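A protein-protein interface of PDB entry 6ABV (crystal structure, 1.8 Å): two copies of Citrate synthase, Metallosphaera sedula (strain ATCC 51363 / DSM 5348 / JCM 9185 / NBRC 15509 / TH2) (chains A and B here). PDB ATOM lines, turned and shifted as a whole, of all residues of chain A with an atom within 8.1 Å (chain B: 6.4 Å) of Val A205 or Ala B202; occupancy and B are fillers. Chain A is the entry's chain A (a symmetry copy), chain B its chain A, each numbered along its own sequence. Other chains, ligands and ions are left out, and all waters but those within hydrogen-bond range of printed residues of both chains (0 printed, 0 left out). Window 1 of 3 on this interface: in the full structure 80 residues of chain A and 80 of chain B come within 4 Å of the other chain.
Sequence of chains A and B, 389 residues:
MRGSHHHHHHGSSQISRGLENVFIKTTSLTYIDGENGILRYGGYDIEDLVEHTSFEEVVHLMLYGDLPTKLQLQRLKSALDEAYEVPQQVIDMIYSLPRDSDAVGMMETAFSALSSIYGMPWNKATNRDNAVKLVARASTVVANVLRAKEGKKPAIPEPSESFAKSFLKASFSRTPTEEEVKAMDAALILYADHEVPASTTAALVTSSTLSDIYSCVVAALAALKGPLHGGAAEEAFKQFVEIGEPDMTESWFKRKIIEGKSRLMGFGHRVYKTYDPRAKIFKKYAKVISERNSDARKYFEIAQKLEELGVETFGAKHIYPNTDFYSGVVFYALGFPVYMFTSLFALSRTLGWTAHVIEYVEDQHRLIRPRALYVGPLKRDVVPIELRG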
ATOM      1  N   ILE A  24     -23.107 -19.795 -39.378  1.00  0.00           N
ATOM      2  CA  ILE A  24     -23.639 -19.972 -38.025  1.00  0.00           C
ATOM      3  C   ILE A  24     -25.079 -19.462 -37.975  1.00  0.00           C
ATOM      4  O   ILE A  24     -25.829 -19.867 -37.091  1.00  0.00           O
ATOM      5  CB  ILE A  24     -22.773 -19.202 -36.939  1.00  0.00           C
ATOM      6  CG1 ILE A  24     -23.316 -19.405 -35.531  1.00  0.00           C
ATOM      7  CG2 ILE A  24     -22.625 -17.718 -37.285  1.00  0.00           C
ATOM      8  CD1 ILE A  24     -22.265 -19.282 -34.432  1.00  0.00           C
ATOM      9  N   ALA A 198     -14.910 -13.081 -33.716  1.00  0.00           N
ATOM     10  CA  ALA A 198     -15.016 -13.828 -32.540  1.00  0.00           C
ATOM     11  C   ALA A 198     -15.889 -13.108 -31.507  1.00  0.00           C
ATOM     12  O   ALA A 198     -16.526 -13.798 -30.729  1.00  0.00           O
ATOM     13  CB  ALA A 198     -13.637 -14.177 -31.951  1.00  0.00           C
ATOM     14  N   SER A 199     -15.842 -11.793 -31.500  1.00  0.00           N
ATOM     15  CA  SER A 199     -16.693 -11.021 -30.542  1.00  0.00           C
ATOM     16  C   SER A 199     -18.226 -11.293 -30.786  1.00  0.00           C
ATOM     17  O   SER A 199     -18.968 -11.672 -29.888  1.00  0.00           O
ATOM     18  CB  SER A 199     -16.357  -9.582 -30.607  1.00  0.00           C
ATOM     19  OG  SER A 199     -16.450  -8.989 -31.885  1.00  0.00           O
ATOM     20  N   THR A 200     -18.644 -11.185 -32.053  1.00  0.00           N
ATOM     21  CA  THR A 200     -20.026 -11.489 -32.403  1.00  0.00           C
ATOM     22  C   THR A 200     -20.317 -12.942 -32.115  1.00  0.00           C
ATOM     23  O   THR A 200     -21.393 -13.254 -31.625  1.00  0.00           O
ATOM     24  CB  THR A 200     -20.280 -11.127 -33.899  1.00  0.00           C
ATOM     25  OG1 THR A 200     -19.853  -9.822 -34.141  1.00  0.00           O
ATOM     26  CG2 THR A 200     -21.672 -11.310 -34.271  1.00  0.00           C
ATOM     27  N   THR A 201     -19.392 -13.864 -32.399  1.00  0.00           N
ATOM     28  CA  THR A 201     -19.599 -15.259 -32.085  1.00  0.00           C
ATOM     29  C   THR A 201     -19.809 -15.528 -30.580  1.00  0.00           C
ATOM     30  O   THR A 201     -20.711 -16.233 -30.183  1.00  0.00           O
ATOM     31  CB  THR A 201     -18.469 -16.180 -32.673  1.00  0.00           C
ATOM     32  OG1 THR A 201     -18.268 -15.835 -34.063  1.00  0.00           O
ATOM     33  CG2 THR A 201     -18.732 -17.604 -32.471  1.00  0.00           C
ATOM     34  N   ALA A 202     -18.964 -14.856 -29.758  1.00  0.00           N
ATOM     35  CA  ALA A 202     -19.109 -15.033 -28.300  1.00  0.00           C
ATOM     36  C   ALA A 202     -20.471 -14.526 -27.824  1.00  0.00           C
ATOM     37  O   ALA A 202     -21.097 -15.148 -26.985  1.00  0.00           O
ATOM     38  CB  ALA A 202     -17.986 -14.292 -27.570  1.00  0.00           C
ATOM     39  N   ALA A 203     -20.922 -13.399 -28.409  1.00  0.00           N
ATOM     40  CA  ALA A 203     -22.269 -12.886 -28.113  1.00  0.00           C
ATOM     41  C   ALA A 203     -23.368 -13.856 -28.463  1.00  0.00           C
ATOM     42  O   ALA A 203     -24.258 -14.064 -27.713  1.00  0.00           O
ATOM     43  CB  ALA A 203     -22.457 -11.611 -28.784  1.00  0.00           C
ATOM     44  N   LEU A 204     -23.227 -14.461 -29.657  1.00  0.00           N
ATOM     45  CA  LEU A 204     -24.197 -15.450 -30.066  1.00  0.00           C
ATOM     46  C   LEU A 204     -24.272 -16.660 -29.144  1.00  0.00           C
ATOM     47  O   LEU A 204     -25.323 -17.165 -28.834  1.00  0.00           O
ATOM     48  CB  LEU A 204     -23.964 -15.825 -31.554  1.00  0.00           C
ATOM     49  CG  LEU A 204     -24.255 -14.738 -32.575  1.00  0.00           C
ATOM     50  CD1 LEU A 204     -23.609 -15.051 -33.917  1.00  0.00           C
ATOM     51  CD2 LEU A 204     -25.759 -14.519 -32.792  1.00  0.00           C
ATOM     52  N   VAL A 205     -23.115 -17.242 -28.741  1.00  0.00           N
ATOM     53  CA  VAL A 205     -23.084 -18.324 -27.818  1.00  0.00           C
ATOM     54  C   VAL A 205     -23.749 -17.979 -26.526  1.00  0.00           C
ATOM     55  O   VAL A 205     -24.519 -18.747 -25.950  1.00  0.00           O
ATOM     56  CB  VAL A 205     -21.591 -18.793 -27.572  1.00  0.00           C
ATOM     57  CG1 VAL A 205     -21.527 -19.805 -26.509  1.00  0.00           C
ATOM     58  CG2 VAL A 205     -21.053 -19.320 -28.884  1.00  0.00           C
ATOM     59  N   THR A 206     -23.452 -16.772 -26.011  1.00  0.00           N
ATOM     60  CA  THR A 206     -24.021 -16.397 -24.768  1.00  0.00           C
ATOM     61  C   THR A 206     -25.566 -16.197 -24.887  1.00  0.00           C
ATOM     62  O   THR A 206     -26.307 -16.490 -23.982  1.00  0.00           O
ATOM     63  CB  THR A 206     -23.295 -15.112 -24.312  1.00  0.00           C
ATOM     64  OG1 THR A 206     -21.888 -15.403 -24.145  1.00  0.00           O
ATOM     65  CG2 THR A 206     -23.865 -14.615 -23.047  1.00  0.00           C
ATOM     66  N   SER A 207     -26.037 -15.650 -26.013  1.00  0.00           N
ATOM     67  CA  SER A 207     -27.479 -15.450 -26.232  1.00  0.00           C
ATOM     68  C   SER A 207     -28.221 -16.807 -26.353  1.00  0.00           C
ATOM     69  O   SER A 207     -29.386 -16.885 -25.973  1.00  0.00           O
ATOM     70  CB  SER A 207     -27.701 -14.599 -27.465  1.00  0.00           C
ATOM     71  OG  SER A 207     -27.589 -15.337 -28.697  1.00  0.00           O
ATOM     72  N   SER A 208     -27.486 -17.827 -26.812  1.00  0.00           N
ATOM     73  CA  SER A 208     -28.030 -19.213 -26.950  1.00  0.00           C
ATOM     74  C   SER A 208     -28.557 -19.773 -25.644  1.00  0.00           C
ATOM     75  O   SER A 208     -29.459 -20.611 -25.606  1.00  0.00           O
ATOM     76  CB  SER A 208     -27.021 -20.116 -27.639  1.00  0.00           C
ATOM     77  OG  SER A 208     -26.146 -20.757 -26.734  1.00  0.00           O
ATOM     78  N   THR A 209     -28.064 -19.284 -24.501  1.00  0.00           N
ATOM     79  CA  THR A 209     -28.583 -19.705 -23.229  1.00  0.00           C
ATOM     80  C   THR A 209     -29.673 -18.782 -22.681  1.00  0.00           C
ATOM     81  O   THR A 209     -30.114 -19.026 -21.615  1.00  0.00           O
ATOM     82  CB  THR A 209     -27.487 -19.797 -22.153  1.00  0.00           C
ATOM     83  OG1 THR A 209     -27.052 -18.451 -21.815  1.00  0.00           O
ATOM     84  CG2 THR A 209     -26.303 -20.562 -22.712  1.00  0.00           C
ATOM     85  N   LEU A 210     -30.016 -17.712 -23.417  1.00  0.00           N
ATOM     86  CA  LEU A 210     -30.914 -16.655 -23.028  1.00  0.00           C
ATOM     87  C   LEU A 210     -30.339 -15.827 -21.916  1.00  0.00           C
ATOM     88  O   LEU A 210     -31.055 -15.189 -21.211  1.00  0.00           O
ATOM     89  CB  LEU A 210     -32.339 -17.163 -22.674  1.00  0.00           C
ATOM     90  CG  LEU A 210     -32.918 -17.964 -23.826  1.00  0.00           C
ATOM     91  CD1 LEU A 210     -34.317 -18.379 -23.383  1.00  0.00           C
ATOM     92  CD2 LEU A 210     -32.924 -17.263 -25.173  1.00  0.00           C
ATOM     93  N   SER A 211     -28.982 -15.778 -21.811  1.00  0.00           N
ATOM     94  CA  SER A 211     -28.356 -14.735 -20.968  1.00  0.00           C
ATOM     95  C   SER A 211     -28.729 -13.382 -21.522  1.00  0.00           C
ATOM     96  O   SER A 211     -28.913 -13.182 -22.754  1.00  0.00           O
ATOM     97  CB  SER A 211     -26.826 -14.929 -20.995  1.00  0.00           C
ATOM     98  OG  SER A 211     -26.285 -14.056 -20.037  1.00  0.00           O
ATOM     99  N   CYS A 216     -24.414 -10.688 -23.170  1.00  0.00           N
ATOM    100  CA  CYS A 216     -23.980 -11.011 -24.566  1.00  0.00           C
ATOM    101  C   CYS A 216     -22.865 -10.062 -25.002  1.00  0.00           C
ATOM    102  O   CYS A 216     -21.824 -10.443 -25.591  1.00  0.00           O
ATOM    103  CB  CYS A 216     -25.163 -11.037 -25.552  1.00  0.00           C
ATOM    104  SG  CYS A 216     -26.409 -12.227 -25.156  1.00  0.00           S
ATOM    105  N   ALA A 219     -19.502 -10.844 -23.143  1.00  0.00           N
ATOM    106  CA  ALA A 219     -18.785 -11.914 -23.869  1.00  0.00           C
ATOM    107  C   ALA A 219     -18.074 -11.397 -25.097  1.00  0.00           C
ATOM    108  O   ALA A 219     -16.921 -11.718 -25.376  1.00  0.00           O
ATOM    109  CB  ALA A 219     -19.682 -13.068 -24.150  1.00  0.00           C
ATOM    110  N   ALA A 222     -15.006  -9.575 -23.992  1.00  0.00           N
ATOM    111  CA  ALA A 222     -13.973 -10.529 -23.489  1.00  0.00           C
ATOM    112  C   ALA A 222     -13.196 -11.072 -24.700  1.00  0.00           C
ATOM    113  O   ALA A 222     -11.977 -11.133 -24.683  1.00  0.00           O
ATOM    114  CB  ALA A 222     -14.616 -11.667 -22.695  1.00  0.00           C
ATOM    115  N   ALA A 223     -13.946 -11.418 -25.776  1.00  0.00           N
ATOM    116  CA  ALA A 223     -13.254 -11.855 -26.980  1.00  0.00           C
ATOM    117  C   ALA A 223     -12.467 -10.739 -27.671  1.00  0.00           C
ATOM    118  O   ALA A 223     -11.294 -10.954 -28.158  1.00  0.00           O
ATOM    119  CB  ALA A 223     -14.236 -12.555 -27.889  1.00  0.00           C
ATOM    120  N   VAL A 357     -27.713 -10.726 -32.027  1.00  0.00           N
ATOM    121  CA  VAL A 357     -28.247 -11.597 -30.995  1.00  0.00           C
ATOM    122  C   VAL A 357     -29.781 -11.540 -30.968  1.00  0.00           C
ATOM    123  O   VAL A 357     -30.405 -12.594 -30.756  1.00  0.00           O
ATOM    124  CB  VAL A 357     -27.649 -11.455 -29.561  1.00  0.00           C
ATOM    125  CG1 VAL A 357     -26.180 -11.905 -29.572  1.00  0.00           C
ATOM    126  CG2 VAL A 357     -27.798 -10.068 -28.933  1.00  0.00           C
ATOM    127  N   TYR A 360     -30.782 -13.733 -33.864  1.00  0.00           N
ATOM    128  CA  TYR A 360     -30.524 -15.115 -33.509  1.00  0.00           C
ATOM    129  C   TYR A 360     -31.550 -15.669 -32.531  1.00  0.00           C
ATOM    130  O   TYR A 360     -32.138 -16.724 -32.794  1.00  0.00           O
ATOM    131  CB  TYR A 360     -29.111 -15.302 -32.916  1.00  0.00           C
ATOM    132  CG  TYR A 360     -28.776 -16.743 -32.682  1.00  0.00           C
ATOM    133  CD1 TYR A 360     -28.410 -17.541 -33.740  1.00  0.00           C
ATOM    134  CD2 TYR A 360     -28.897 -17.315 -31.414  1.00  0.00           C
ATOM    135  CE1 TYR A 360     -28.075 -18.877 -33.522  1.00  0.00           C
ATOM    136  CE2 TYR A 360     -28.637 -18.666 -31.201  1.00  0.00           C
ATOM    137  CZ  TYR A 360     -28.221 -19.444 -32.262  1.00  0.00           C
ATOM    138  OH  TYR A 360     -27.911 -20.791 -32.046  1.00  0.00           O
ATOM    139  N   HIS A 365     -33.269 -19.627 -32.832  1.00  0.00           N
ATOM    140  CA  HIS A 365     -32.694 -20.022 -31.555  1.00  0.00           C
ATOM    141  C   HIS A 365     -32.396 -21.522 -31.515  1.00  0.00           C
ATOM    142  O   HIS A 365     -33.173 -22.328 -32.012  1.00  0.00           O
ATOM    143  CB  HIS A 365     -33.591 -19.645 -30.367  1.00  0.00           C
ATOM    144  CG  HIS A 365     -33.033 -20.070 -29.039  1.00  0.00           C
ATOM    145  ND1 HIS A 365     -33.397 -21.242 -28.426  1.00  0.00           N
ATOM    146  CD2 HIS A 365     -32.085 -19.512 -28.245  1.00  0.00           C
ATOM    147  CE1 HIS A 365     -32.720 -21.383 -27.302  1.00  0.00           C
ATOM    148  NE2 HIS A 365     -31.918 -20.345 -27.168  1.00  0.00           N
ATOM    149  N   ARG A 366     -31.234 -21.865 -30.967  1.00  0.00           N
ATOM    150  CA  ARG A 366     -31.034 -23.176 -30.338  1.00  0.00           C
ATOM    151  C   ARG A 366     -29.867 -23.051 -29.373  1.00  0.00           C
ATOM    152  O   ARG A 366     -28.989 -22.239 -29.611  1.00  0.00           O
ATOM    153  CB  ARG A 366     -30.778 -24.288 -31.360  1.00  0.00           C
ATOM    154  CG  ARG A 366     -29.667 -24.003 -32.350  1.00  0.00           C
ATOM    155  CD  ARG A 366     -29.496 -25.144 -33.350  1.00  0.00           C
ATOM    156  NE  ARG A 366     -28.083 -25.359 -33.693  1.00  0.00           N
ATOM    157  CZ  ARG A 366     -27.628 -25.850 -34.847  1.00  0.00           C
ATOM    158  NH1 ARG A 366     -28.444 -26.197 -35.844  1.00  0.00           N
ATOM    159  NH2 ARG A 366     -26.318 -25.981 -35.012  1.00  0.00           N
ATOM    160  N   LEU A 367     -29.879 -23.843 -28.298  1.00  0.00           N
ATOM    161  CA  LEU A 367     -28.729 -23.906 -27.375  1.00  0.00           C
ATOM    162  C   LEU A 367     -27.470 -24.371 -28.129  1.00  0.00           C
ATOM    163  O   LEU A 367     -27.525 -25.334 -28.893  1.00  0.00           O
ATOM    164  CB  LEU A 367     -29.019 -24.848 -26.208  1.00  0.00           C
ATOM    165  CG  LEU A 367     -28.087 -24.828 -24.988  1.00  0.00           C
ATOM    166  CD1 LEU A 367     -28.224 -23.549 -24.156  1.00  0.00           C
ATOM    167  CD2 LEU A 367     -28.379 -26.024 -24.107  1.00  0.00           C
ATOM    168  N   ILE A 368     -26.356 -23.652 -27.954  1.00  0.00           N
ATOM    169  CA  ILE A 368     -25.122 -23.987 -28.655  1.00  0.00           C
ATOM    170  C   ILE A 368     -24.433 -24.971 -27.683  1.00  0.00           C
ATOM    171  O   ILE A 368     -24.134 -24.605 -26.540  1.00  0.00           O
ATOM    172  CB  ILE A 368     -24.317 -22.716 -29.087  1.00  0.00           C
ATOM    173  CG1 ILE A 368     -25.095 -21.963 -30.193  1.00  0.00           C
ATOM    174  CG2 ILE A 368     -22.934 -23.089 -29.604  1.00  0.00           C
ATOM    175  CD1 ILE A 368     -24.567 -20.609 -30.662  1.00  0.00           C
ATOM    176  N   ARG A 369     -24.294 -26.244 -28.116  1.00  0.00           N
ATOM    177  CA  ARG A 369     -23.619 -27.305 -27.350  1.00  0.00           C
ATOM    178  C   ARG A 369     -22.851 -28.301 -28.270  1.00  0.00           C
ATOM    179  O   ARG A 369     -23.360 -29.400 -28.554  1.00  0.00           O
ATOM    180  CB  ARG A 369     -24.626 -28.047 -26.432  1.00  0.00           C
ATOM    181  CG  ARG A 369     -25.983 -28.395 -27.050  1.00  0.00           C
ATOM    182  CD  ARG A 369     -26.893 -29.138 -26.069  1.00  0.00           C
ATOM    183  NE  ARG A 369     -28.308 -29.043 -26.454  1.00  0.00           N
ATOM    184  CZ  ARG A 369     -29.352 -29.419 -25.706  1.00  0.00           C
ATOM    185  NH1 ARG A 369     -29.175 -29.941 -24.498  1.00  0.00           N
ATOM    186  NH2 ARG A 369     -30.596 -29.267 -26.168  1.00  0.00           N
ATOM    187  N   PRO A 370     -21.634 -27.921 -28.743  1.00  0.00           N
ATOM    188  CA  PRO A 370     -20.809 -28.854 -29.551  1.00  0.00           C
ATOM    189  C   PRO A 370     -20.202 -29.993 -28.731  1.00  0.00           C
ATOM    190  O   PRO A 370     -20.638 -30.264 -27.594  1.00  0.00           O
ATOM    191  CB  PRO A 370     -19.733 -27.942 -30.126  1.00  0.00           C
ATOM    192  CG  PRO A 370     -19.577 -26.852 -29.128  1.00  0.00           C
ATOM    193  CD  PRO A 370     -20.921 -26.656 -28.501  1.00  0.00           C
ATOM    194  N   PRO B 197     -20.624 -27.610 -22.740  1.00  0.00           N
ATOM    195  CA  PRO B 197     -21.806 -26.691 -22.660  1.00  0.00           C
ATOM    196  C   PRO B 197     -21.490 -25.263 -23.150  1.00  0.00           C
ATOM    197  O   PRO B 197     -20.375 -24.953 -23.526  1.00  0.00           O
ATOM    198  CB  PRO B 197     -22.215 -26.798 -21.231  1.00  0.00           C
ATOM    199  CG  PRO B 197     -20.967 -27.098 -20.480  1.00  0.00           C
ATOM    200  CD  PRO B 197     -20.130 -27.986 -21.409  1.00  0.00           C
ATOM    201  N   ALA B 198     -22.514 -24.406 -23.232  1.00  0.00           N
ATOM    202  CA  ALA B 198     -22.342 -23.142 -23.803  1.00  0.00           C
ATOM    203  C   ALA B 198     -21.276 -22.340 -23.050  1.00  0.00           C
ATOM    204  O   ALA B 198     -20.624 -21.531 -23.689  1.00  0.00           O
ATOM    205  CB  ALA B 198     -23.666 -22.360 -23.884  1.00  0.00           C
ATOM    206  N   SER B 199     -21.181 -22.543 -21.753  1.00  0.00           N
ATOM    207  CA  SER B 199     -20.140 -21.819 -20.958  1.00  0.00           C
ATOM    208  C   SER B 199     -18.688 -22.177 -21.453  1.00  0.00           C
ATOM    209  O   SER B 199     -17.884 -21.314 -21.782  1.00  0.00           O
ATOM    210  CB  SER B 199     -20.327 -22.083 -19.515  1.00  0.00           C
ATOM    211  OG  SER B 199     -20.332 -23.444 -19.137  1.00  0.00           O
ATOM    212  N   THR B 200     -18.422 -23.482 -21.589  1.00  0.00           N
ATOM    213  CA  THR B 200     -17.135 -23.923 -22.112  1.00  0.00           C
ATOM    214  C   THR B 200     -16.966 -23.433 -23.530  1.00  0.00           C
ATOM    215  O   THR B 200     -15.876 -23.016 -23.897  1.00  0.00           O
ATOM    216  CB  THR B 200     -17.032 -25.476 -22.013  1.00  0.00           C
ATOM    217  OG1 THR B 200     -17.344 -25.882 -20.716  1.00  0.00           O
ATOM    218  CG2 THR B 200     -15.725 -25.959 -22.422  1.00  0.00           C
ATOM    219  N   THR B 201     -18.012 -23.463 -24.363  1.00  0.00           N
ATOM    220  CA  THR B 201     -17.917 -22.949 -25.709  1.00  0.00           C
ATOM    221  C   THR B 201     -17.551 -21.451 -25.773  1.00  0.00           C
ATOM    222  O   THR B 201     -16.687 -21.042 -26.518  1.00  0.00           O
ATOM    223  CB  THR B 201     -19.203 -23.255 -26.560  1.00  0.00           C
ATOM    224  OG1 THR B 201     -19.538 -24.654 -26.404  1.00  0.00           O
ATOM    225  CG2 THR B 201     -19.070 -22.852 -27.959  1.00  0.00           C
ATOM    226  N   ALA B 202     -18.210 -20.665 -24.886  1.00  0.00           N
ATOM    227  CA  ALA B 202     -17.905 -19.221 -24.858  1.00  0.00           C
ATOM    228  C   ALA B 202     -16.447 -18.982 -24.459  1.00  0.00           C
ATOM    229  O   ALA B 202     -15.792 -18.124 -25.022  1.00  0.00           O
ATOM    230  CB  ALA B 202     -18.842 -18.507 -23.882  1.00  0.00           C
ATOM    231  N   ALA B 203     -15.956 -19.788 -23.498  1.00  0.00           N
ATOM    232  CA  ALA B 203     -14.535 -19.726 -23.118  1.00  0.00           C
ATOM    233  C   ALA B 203     -13.598 -20.027 -24.259  1.00  0.00           C
ATOM    234  O   ALA B 203     -12.648 -19.351 -24.462  1.00  0.00           O
ATOM    235  CB  ALA B 203     -14.298 -20.611 -21.992  1.00  0.00           C
ATOM    236  N   LEU B 204     -13.950 -21.084 -25.014  1.00  0.00           N
ATOM    237  CA  LEU B 204     -13.150 -21.427 -26.167  1.00  0.00           C
ATOM    238  C   LEU B 204     -13.090 -20.332 -27.225  1.00  0.00           C
ATOM    239  O   LEU B 204     -12.068 -20.057 -27.804  1.00  0.00           O
ATOM    240  CB  LEU B 204     -13.605 -22.799 -26.729  1.00  0.00           C
ATOM    241  CG  LEU B 204     -13.330 -24.010 -25.852  1.00  0.00           C
ATOM    242  CD1 LEU B 204     -14.168 -25.206 -26.280  1.00  0.00           C
ATOM    243  CD2 LEU B 204     -11.850 -24.419 -25.857  1.00  0.00           C
ATOM    244  N   VAL B 205     -14.242 -19.719 -27.591  1.00  0.00           N
ATOM    245  CA  VAL B 205     -14.273 -18.634 -28.509  1.00  0.00           C
ATOM    246  C   VAL B 205     -13.419 -17.493 -28.061  1.00  0.00           C
ATOM    247  O   VAL B 205     -12.670 -16.884 -28.823  1.00  0.00           O
ATOM    248  CB  VAL B 205     -15.765 -18.156 -28.747  1.00  0.00           C
ATOM    249  CG1 VAL B 205     -15.803 -16.941 -29.571  1.00  0.00           C
ATOM    250  CG2 VAL B 205     -16.515 -19.300 -29.393  1.00  0.00           C
ATOM    251  N   THR B 206     -13.520 -17.154 -26.762  1.00  0.00           N
ATOM    252  CA  THR B 206     -12.763 -16.056 -26.279  1.00  0.00           C
ATOM    253  C   THR B 206     -11.233 -16.370 -26.294  1.00  0.00           C
ATOM    254  O   THR B 206     -10.420 -15.513 -26.537  1.00  0.00           O
ATOM    255  CB  THR B 206     -13.286 -15.742 -24.860  1.00  0.00           C
ATOM    256  OG1 THR B 206     -14.684 -15.381 -24.944  1.00  0.00           O
ATOM    257  CG2 THR B 206     -12.513 -14.644 -24.254  1.00  0.00           C
ATOM    258  N   SER B 207     -10.851 -17.614 -25.985  1.00  0.00           N
ATOM    259  CA  SER B 207      -9.434 -18.014 -26.001  1.00  0.00           C
ATOM    260  C   SER B 207      -8.861 -17.991 -27.443  1.00  0.00           C
ATOM    261  O   SER B 207      -7.673 -17.729 -27.607  1.00  0.00           O
ATOM    262  CB  SER B 207      -9.278 -19.387 -25.379  1.00  0.00           C
ATOM    263  OG  SER B 207      -9.621 -20.463 -26.273  1.00  0.00           O
ATOM    264  N   SER B 215     -10.557 -13.478 -18.647  1.00  0.00           N
ATOM    265  CA  SER B 215     -11.630 -13.118 -19.635  1.00  0.00           C
ATOM    266  C   SER B 215     -12.308 -14.359 -20.317  1.00  0.00           C
ATOM    267  O   SER B 215     -13.536 -14.277 -20.586  1.00  0.00           O
ATOM    268  CB  SER B 215     -11.156 -12.078 -20.682  1.00  0.00           C
ATOM    269  OG  SER B 215     -11.213 -10.757 -20.150  1.00  0.00           O
ATOM    270  N   CYS B 216     -11.569 -15.464 -20.488  1.00  0.00           N
ATOM    271  CA  CYS B 216     -12.206 -16.735 -20.961  1.00  0.00           C
ATOM    272  C   CYS B 216     -13.260 -17.199 -19.956  1.00  0.00           C
ATOM    273  O   CYS B 216     -14.400 -17.604 -20.289  1.00  0.00           O
ATOM    274  CB  CYS B 216     -11.165 -17.824 -21.282  1.00  0.00           C
ATOM    275  SG  CYS B 216     -10.013 -17.373 -22.545  1.00  0.00           S
ATOM    276  N   ALA B 219     -16.428 -14.890 -20.025  1.00  0.00           N
ATOM    277  CA  ALA B 219     -17.340 -15.351 -21.095  1.00  0.00           C
ATOM    278  C   ALA B 219     -18.139 -16.565 -20.683  1.00  0.00           C
ATOM    279  O   ALA B 219     -19.346 -16.662 -20.896  1.00  0.00           O
ATOM    280  CB  ALA B 219     -16.612 -15.534 -22.380  1.00  0.00           C
ATOM    281  N   ALA B 220     -17.488 -17.523 -20.055  1.00  0.00           N
ATOM    282  CA  ALA B 220     -18.164 -18.668 -19.572  1.00  0.00           C
ATOM    283  C   ALA B 220     -19.238 -18.384 -18.567  1.00  0.00           C
ATOM    284  O   ALA B 220     -20.371 -18.925 -18.624  1.00  0.00           O
ATOM    285  CB  ALA B 220     -17.144 -19.668 -19.002  1.00  0.00           C
ATOM    286  N   LEU B 221     -18.963 -17.449 -17.631  1.00  0.00           N
ATOM    287  CA  LEU B 221     -19.975 -17.004 -16.724  1.00  0.00           C
ATOM    288  C   LEU B 221     -21.107 -16.282 -17.355  1.00  0.00           C
ATOM    289  O   LEU B 221     -22.261 -16.441 -16.938  1.00  0.00           O
ATOM    290  CB  LEU B 221     -19.259 -16.159 -15.635  1.00  0.00           C
ATOM    291  CG  LEU B 221     -18.324 -16.913 -14.667  1.00  0.00           C
ATOM    292  CD1 LEU B 221     -17.400 -15.897 -13.955  1.00  0.00           C
ATOM    293  CD2 LEU B 221     -19.051 -17.850 -13.698  1.00  0.00           C
ATOM    294  N   ALA B 223     -22.298 -16.788 -20.291  1.00  0.00           N
ATOM    295  CA  ALA B 223     -23.178 -17.824 -20.813  1.00  0.00           C
ATOM    296  C   ALA B 223     -23.921 -18.600 -19.724  1.00  0.00           C
ATOM    297  O   ALA B 223     -25.163 -18.918 -19.862  1.00  0.00           O
ATOM    298  CB  ALA B 223     -22.396 -18.706 -21.759  1.00  0.00           C
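The backbone carbonyl oxygen of Ala B223 lies within hydrogen-bond range of the side-chain hydroxyl of Thr A209 (2.8 Å).
Ala A198 touches Val B205, and with the chains exchanged Val A205 touches Ala B198.
Ala A202 touches Val B205, and with the chains exchanged Val A205 touches Ala B202.
Thr A206 touches Ala B223, and with the chains exchanged Ala A223 touches Thr B206.
Among the printed residues, pairs that only touch across the chains: Pro A370 with Thr B201 (3.2 Å), Thr A209 with Ala B198 (3.4 Å), Ala A198 with Val B205 (3.4 Å), Val A205 with Ala B198 (3.4 Å), Ile A368 with Ala B198 (3.5 Å), Ala A222 with Ser B215 (3.5 Å), Ala A222 with Thr B206 (3.6 Å), Ala A202 with Val B205 (3.8 Å), Val A205 with Ala B202 (3.8 Å), Thr A206 with Ala B223 (3.8 Å) and Ala A223 with Thr B206 (3.8 Å).
Val A205 touches two residues of chain B.
Cys A216 touches none of the printed residues of chain B.
Of the printed residues of chain B, Ala A223 touches Thr B206.
Of the printed residues of chain A, Thr B201 touches Pro A370.
Of chain A, only Val A205 comes within 4 Å of Ala B202.
No residue of chain A comes within 4 Å of Ala B203.
Of the printed residues of chain A, Val B205 touches Ala A198 (3.4 Å) and Ala A202 (3.8 Å).
The nearest printed residue of chain B that does not touch Thr A206 is Ala B219 (4.3 Å).
The side-chain hydroxyl of Thr B206 is in hydrogen-bond range of the backbone carbonyl oxygen of Ala B202 (3.0 Å).
OG of Ser A208 sits at hydrogen-bond distance from O of Val A205 (2.7 Å).
OG1 of Thr B201 lies within hydrogen-bond range of O of Pro B197.
The backbone NH of Ser A211 sits close to the side-chain hydroxyl of Thr A209, at 3.3 Å.
O of Ala A202 is in hydrogen-bond range of OG1 of Thr A206 (3.0 Å).
O of Thr A206 is in hydrogen-bond range of OG1 of Thr A209 (3.0 Å).
Printed residues of chain B that touch a printed residue of chain A: Ala B198, Thr B201, Ala B202, Val B205, Thr B206, Ser B215 and Ala B223.
Hydrophobic or aromatic side chains of chain A that line the printed part of chain B: Ala A202, Val A205, Ala A222 and Pro A370.
Along chain A the printed residues that touch a printed residue of chain B span positions 198 to 370.
Among the printed residues, 12 pairs touch across the chains.
Among the printed residues, no Asp or Glu carboxylate lies within 4 Å of a Lys or Arg side-chain nitrogen of the other chain.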
